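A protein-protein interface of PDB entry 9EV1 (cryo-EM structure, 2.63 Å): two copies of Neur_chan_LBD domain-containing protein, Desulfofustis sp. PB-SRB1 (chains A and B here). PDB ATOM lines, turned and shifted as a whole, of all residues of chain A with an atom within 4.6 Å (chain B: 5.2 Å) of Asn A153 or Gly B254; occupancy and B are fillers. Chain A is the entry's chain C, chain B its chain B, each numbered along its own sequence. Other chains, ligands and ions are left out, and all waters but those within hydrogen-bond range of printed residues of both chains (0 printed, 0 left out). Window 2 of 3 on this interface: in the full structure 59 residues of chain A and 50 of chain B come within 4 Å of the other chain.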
ATOM      1  N   THR A 152     -27.032  -4.032 -19.559  1.00  0.00           N
ATOM      2  CA  THR A 152     -25.925  -4.810 -19.019  1.00  0.00           C
ATOM      3  C   THR A 152     -25.567  -5.939 -19.973  1.00  0.00           C
ATOM      4  O   THR A 152     -26.317  -6.264 -20.897  1.00  0.00           O
ATOM      5  CB  THR A 152     -26.259  -5.399 -17.641  1.00  0.00           C
ATOM      6  OG1 THR A 152     -27.464  -6.166 -17.723  1.00  0.00           O
ATOM      7  CG2 THR A 152     -26.430  -4.304 -16.607  1.00  0.00           C
ATOM      8  N   ASN A 153     -24.399  -6.527 -19.737  1.00  0.00           N
ATOM      9  CA  ASN A 153     -23.947  -7.732 -20.418  1.00  0.00           C
ATOM     10  C   ASN A 153     -23.863  -8.866 -19.403  1.00  0.00           C
ATOM     11  O   ASN A 153     -23.414  -8.657 -18.274  1.00  0.00           O
ATOM     12  CB  ASN A 153     -22.588  -7.511 -21.082  1.00  0.00           C
ATOM     13  CG  ASN A 153     -22.073  -8.746 -21.785  1.00  0.00           C
ATOM     14  OD1 ASN A 153     -22.527  -9.086 -22.876  1.00  0.00           O
ATOM     15  ND2 ASN A 153     -21.113  -9.422 -21.169  1.00  0.00           N
ATOM     16  N   GLN A 154     -24.309 -10.058 -19.802  1.00  0.00           N
ATOM     17  CA  GLN A 154     -24.343 -11.211 -18.908  1.00  0.00           C
ATOM     18  C   GLN A 154     -23.747 -12.454 -19.561  1.00  0.00           C
ATOM     19  O   GLN A 154     -24.192 -13.569 -19.293  1.00  0.00           O
ATOM     20  CB  GLN A 154     -25.768 -11.497 -18.445  1.00  0.00           C
ATOM     21  CG  GLN A 154     -26.394 -10.393 -17.620  1.00  0.00           C
ATOM     22  CD  GLN A 154     -27.867 -10.628 -17.356  1.00  0.00           C
ATOM     23  OE1 GLN A 154     -28.630 -10.937 -18.269  1.00  0.00           O
ATOM     24  NE2 GLN A 154     -28.272 -10.488 -16.100  1.00  0.00           N
ATOM     25  N   ARG A 155     -22.744 -12.285 -20.421  1.00  0.00           N
ATOM     26  CA  ARG A 155     -22.113 -13.404 -21.107  1.00  0.00           C
ATOM     27  C   ARG A 155     -20.602 -13.221 -21.118  1.00  0.00           C
ATOM     28  O   ARG A 155     -20.094 -12.100 -21.039  1.00  0.00           O
ATOM     29  CB  ARG A 155     -22.626 -13.546 -22.549  1.00  0.00           C
ATOM     30  CG  ARG A 155     -24.120 -13.792 -22.655  1.00  0.00           C
ATOM     31  CD  ARG A 155     -24.594 -13.767 -24.097  1.00  0.00           C
ATOM     32  NE  ARG A 155     -24.113 -14.913 -24.859  1.00  0.00           N
ATOM     33  CZ  ARG A 155     -24.463 -15.178 -26.110  1.00  0.00           C
ATOM     34  NH1 ARG A 155     -25.298 -14.398 -26.775  1.00  0.00           N
ATOM     35  NH2 ARG A 155     -23.964 -16.257 -26.708  1.00  0.00           N
ATOM     36  N   LYS A 158     -19.250 -13.811 -25.707  1.00  0.00           N
ATOM     37  CA  LYS A 158     -19.316 -12.654 -26.585  1.00  0.00           C
ATOM     38  C   LYS A 158     -19.966 -11.509 -25.828  1.00  0.00           C
ATOM     39  O   LYS A 158     -20.616 -11.709 -24.798  1.00  0.00           O
ATOM     40  CB  LYS A 158     -20.087 -12.961 -27.873  1.00  0.00           C
ATOM     41  CG  LYS A 158     -21.544 -13.322 -27.653  1.00  0.00           C
ATOM     42  CD  LYS A 158     -22.261 -13.539 -28.973  1.00  0.00           C
ATOM     43  CE  LYS A 158     -21.639 -14.677 -29.763  1.00  0.00           C
ATOM     44  NZ  LYS A 158     -22.354 -14.913 -31.047  1.00  0.00           N
ATOM     45  N   PHE A 159     -19.786 -10.299 -26.347  1.00  0.00           N
ATOM     46  CA  PHE A 159     -20.316  -9.093 -25.728  1.00  0.00           C
ATOM     47  C   PHE A 159     -21.601  -8.688 -26.437  1.00  0.00           C
ATOM     48  O   PHE A 159     -21.603  -8.474 -27.653  1.00  0.00           O
ATOM     49  CB  PHE A 159     -19.287  -7.965 -25.779  1.00  0.00           C
ATOM     50  CG  PHE A 159     -19.686  -6.742 -25.009  1.00  0.00           C
ATOM     51  CD1 PHE A 159     -19.481  -6.670 -23.645  1.00  0.00           C
ATOM     52  CD2 PHE A 159     -20.256  -5.658 -25.652  1.00  0.00           C
ATOM     53  CE1 PHE A 159     -19.847  -5.545 -22.934  1.00  0.00           C
ATOM     54  CE2 PHE A 159     -20.621  -4.531 -24.948  1.00  0.00           C
ATOM     55  CZ  PHE A 159     -20.416  -4.474 -23.588  1.00  0.00           C
ATOM     56  N   GLN A 160     -22.692  -8.585 -25.676  1.00  0.00           N
ATOM     57  CA  GLN A 160     -24.000  -8.232 -26.229  1.00  0.00           C
ATOM     58  C   GLN A 160     -24.819  -7.540 -25.147  1.00  0.00           C
ATOM     59  O   GLN A 160     -25.407  -8.203 -24.279  1.00  0.00           O
ATOM     60  CB  GLN A 160     -24.732  -9.460 -26.762  1.00  0.00           C
ATOM     61  CG  GLN A 160     -26.137  -9.175 -27.267  1.00  0.00           C
ATOM     62  CD  GLN A 160     -26.156  -8.199 -28.428  1.00  0.00           C
ATOM     63  OE1 GLN A 160     -25.298  -8.248 -29.308  1.00  0.00           O
ATOM     64  NE2 GLN A 160     -27.135  -7.302 -28.430  1.00  0.00           N
ATOM     65  N   PRO A 161     -24.880  -6.209 -25.160  1.00  0.00           N
ATOM     66  CA  PRO A 161     -25.712  -5.504 -24.177  1.00  0.00           C
ATOM     67  C   PRO A 161     -27.194  -5.692 -24.463  1.00  0.00           C
ATOM     68  O   PRO A 161     -27.636  -5.633 -25.611  1.00  0.00           O
ATOM     69  CB  PRO A 161     -25.289  -4.039 -24.342  1.00  0.00           C
ATOM     70  CG  PRO A 161     -24.781  -3.955 -25.736  1.00  0.00           C
ATOM     71  CD  PRO A 161     -24.138  -5.278 -26.027  1.00  0.00           C
ATOM     72  N   THR B 250     -14.926  -6.735 -16.973  1.00  0.00           N
ATOM     73  CA  THR B 250     -16.199  -7.089 -16.364  1.00  0.00           C
ATOM     74  C   THR B 250     -15.949  -7.990 -15.164  1.00  0.00           C
ATOM     75  O   THR B 250     -14.862  -8.550 -14.999  1.00  0.00           O
ATOM     76  CB  THR B 250     -17.136  -7.804 -17.350  1.00  0.00           C
ATOM     77  OG1 THR B 250     -16.536  -9.032 -17.780  1.00  0.00           O
ATOM     78  CG2 THR B 250     -17.423  -6.930 -18.563  1.00  0.00           C
ATOM     79  N   ASP B 251     -16.970  -8.127 -14.324  1.00  0.00           N
ATOM     80  CA  ASP B 251     -16.896  -9.012 -13.171  1.00  0.00           C
ATOM     81  C   ASP B 251     -17.136 -10.452 -13.622  1.00  0.00           C
ATOM     82  O   ASP B 251     -17.195 -10.754 -14.816  1.00  0.00           O
ATOM     83  CB  ASP B 251     -17.892  -8.577 -12.100  1.00  0.00           C
ATOM     84  CG  ASP B 251     -19.324  -8.899 -12.471  1.00  0.00           C
ATOM     85  OD1 ASP B 251     -19.664  -8.814 -13.671  1.00  0.00           O
ATOM     86  OD2 ASP B 251     -20.108  -9.246 -11.561  1.00  0.00           O
ATOM     87  N   SER B 252     -17.278 -11.364 -12.659  1.00  0.00           N
ATOM     88  CA  SER B 252     -17.529 -12.764 -12.977  1.00  0.00           C
ATOM     89  C   SER B 252     -18.928 -13.005 -13.528  1.00  0.00           C
ATOM     90  O   SER B 252     -19.155 -14.047 -14.150  1.00  0.00           O
ATOM     91  CB  SER B 252     -17.309 -13.633 -11.739  1.00  0.00           C
ATOM     92  OG  SER B 252     -15.952 -13.612 -11.336  1.00  0.00           O
ATOM     93  N   GLY B 253     -19.861 -12.080 -13.319  1.00  0.00           N
ATOM     94  CA  GLY B 253     -21.205 -12.234 -13.837  1.00  0.00           C
ATOM     95  C   GLY B 253     -21.398 -11.561 -15.179  1.00  0.00           C
ATOM     96  O   GLY B 253     -22.422 -11.756 -15.839  1.00  0.00           O
ATOM     97  N   GLY B 254     -20.415 -10.767 -15.593  1.00  0.00           N
ATOM     98  CA  GLY B 254     -20.473 -10.051 -16.849  1.00  0.00           C
ATOM     99  C   GLY B 254     -20.847  -8.590 -16.742  1.00  0.00           C
ATOM    100  O   GLY B 254     -20.922  -7.913 -17.774  1.00  0.00           O
ATOM    101  N   LYS B 255     -21.085  -8.085 -15.538  1.00  0.00           N
ATOM    102  CA  LYS B 255     -21.451  -6.682 -15.370  1.00  0.00           C
ATOM    103  C   LYS B 255     -20.270  -5.794 -15.748  1.00  0.00           C
ATOM    104  O   LYS B 255     -19.178  -5.955 -15.192  1.00  0.00           O
ATOM    105  CB  LYS B 255     -21.871  -6.421 -13.925  1.00  0.00           C
ATOM    106  CG  LYS B 255     -23.096  -5.538 -13.769  1.00  0.00           C
ATOM    107  CD  LYS B 255     -22.777  -4.077 -14.020  1.00  0.00           C
ATOM    108  CE  LYS B 255     -24.021  -3.217 -13.871  1.00  0.00           C
ATOM    109  NZ  LYS B 255     -24.670  -3.420 -12.547  1.00  0.00           N
ATOM    110  N   PRO B 256     -20.441  -4.858 -16.680  1.00  0.00           N
ATOM    111  CA  PRO B 256     -19.311  -4.018 -17.094  1.00  0.00           C
ATOM    112  C   PRO B 256     -18.828  -3.119 -15.968  1.00  0.00           C
ATOM    113  O   PRO B 256     -19.611  -2.626 -15.152  1.00  0.00           O
ATOM    114  CB  PRO B 256     -19.886  -3.196 -18.254  1.00  0.00           C
ATOM    115  CG  PRO B 256     -21.360  -3.217 -18.039  1.00  0.00           C
ATOM    116  CD  PRO B 256     -21.667  -4.549 -17.432  1.00  0.00           C
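Lys B255 touches Thr A152. N of Lys B255 touches O of Asn A153 (3.6 Å). Gly B253 touches Gln A154 (O to CA, 3.7 Å).
No position is printed for both chains.
Among the printed residues, no Asp or Glu carboxylate lies within 4 Å of a Lys or Arg side-chain nitrogen of the other chain.
Gly B254 touches just one residue of chain A: Asn A153. Printed residues of chain A within 4 Å of Gly B253: Gln A154. Of the printed residues of chain B, Gln A154 touches Gly B253. Printed residues of chain A within 4 Å of Lys B255: Thr A152 and Asn A153.
The backbone carbonyl oxygen of Asn A153 sits close to the backbone carbonyl oxygen of Gly B254, at 2.6 Å.
The side-chain carboxylate (OD1) of Asp B251 sits close to the backbone NH (N) of Gly B253, 3.3 Å away. The side-chain carboxylate (OD1) of Asp B251 sits at hydrogen-bond distance from the backbone NH (N) of Gly B254, at 2.8 Å. OD1 of Asp B251 sits at hydrogen-bond distance from N of Lys B255, at 2.5 Å. The side-chain amide nitrogen of Asn A153 lies within hydrogen-bond range of the backbone carbonyl oxygen of Arg A155, at 2.9 Å. The side-chain amide oxygen of Asn A153 is in hydrogen-bond range of the backbone NH of Gln A160, at 2.8 Å.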
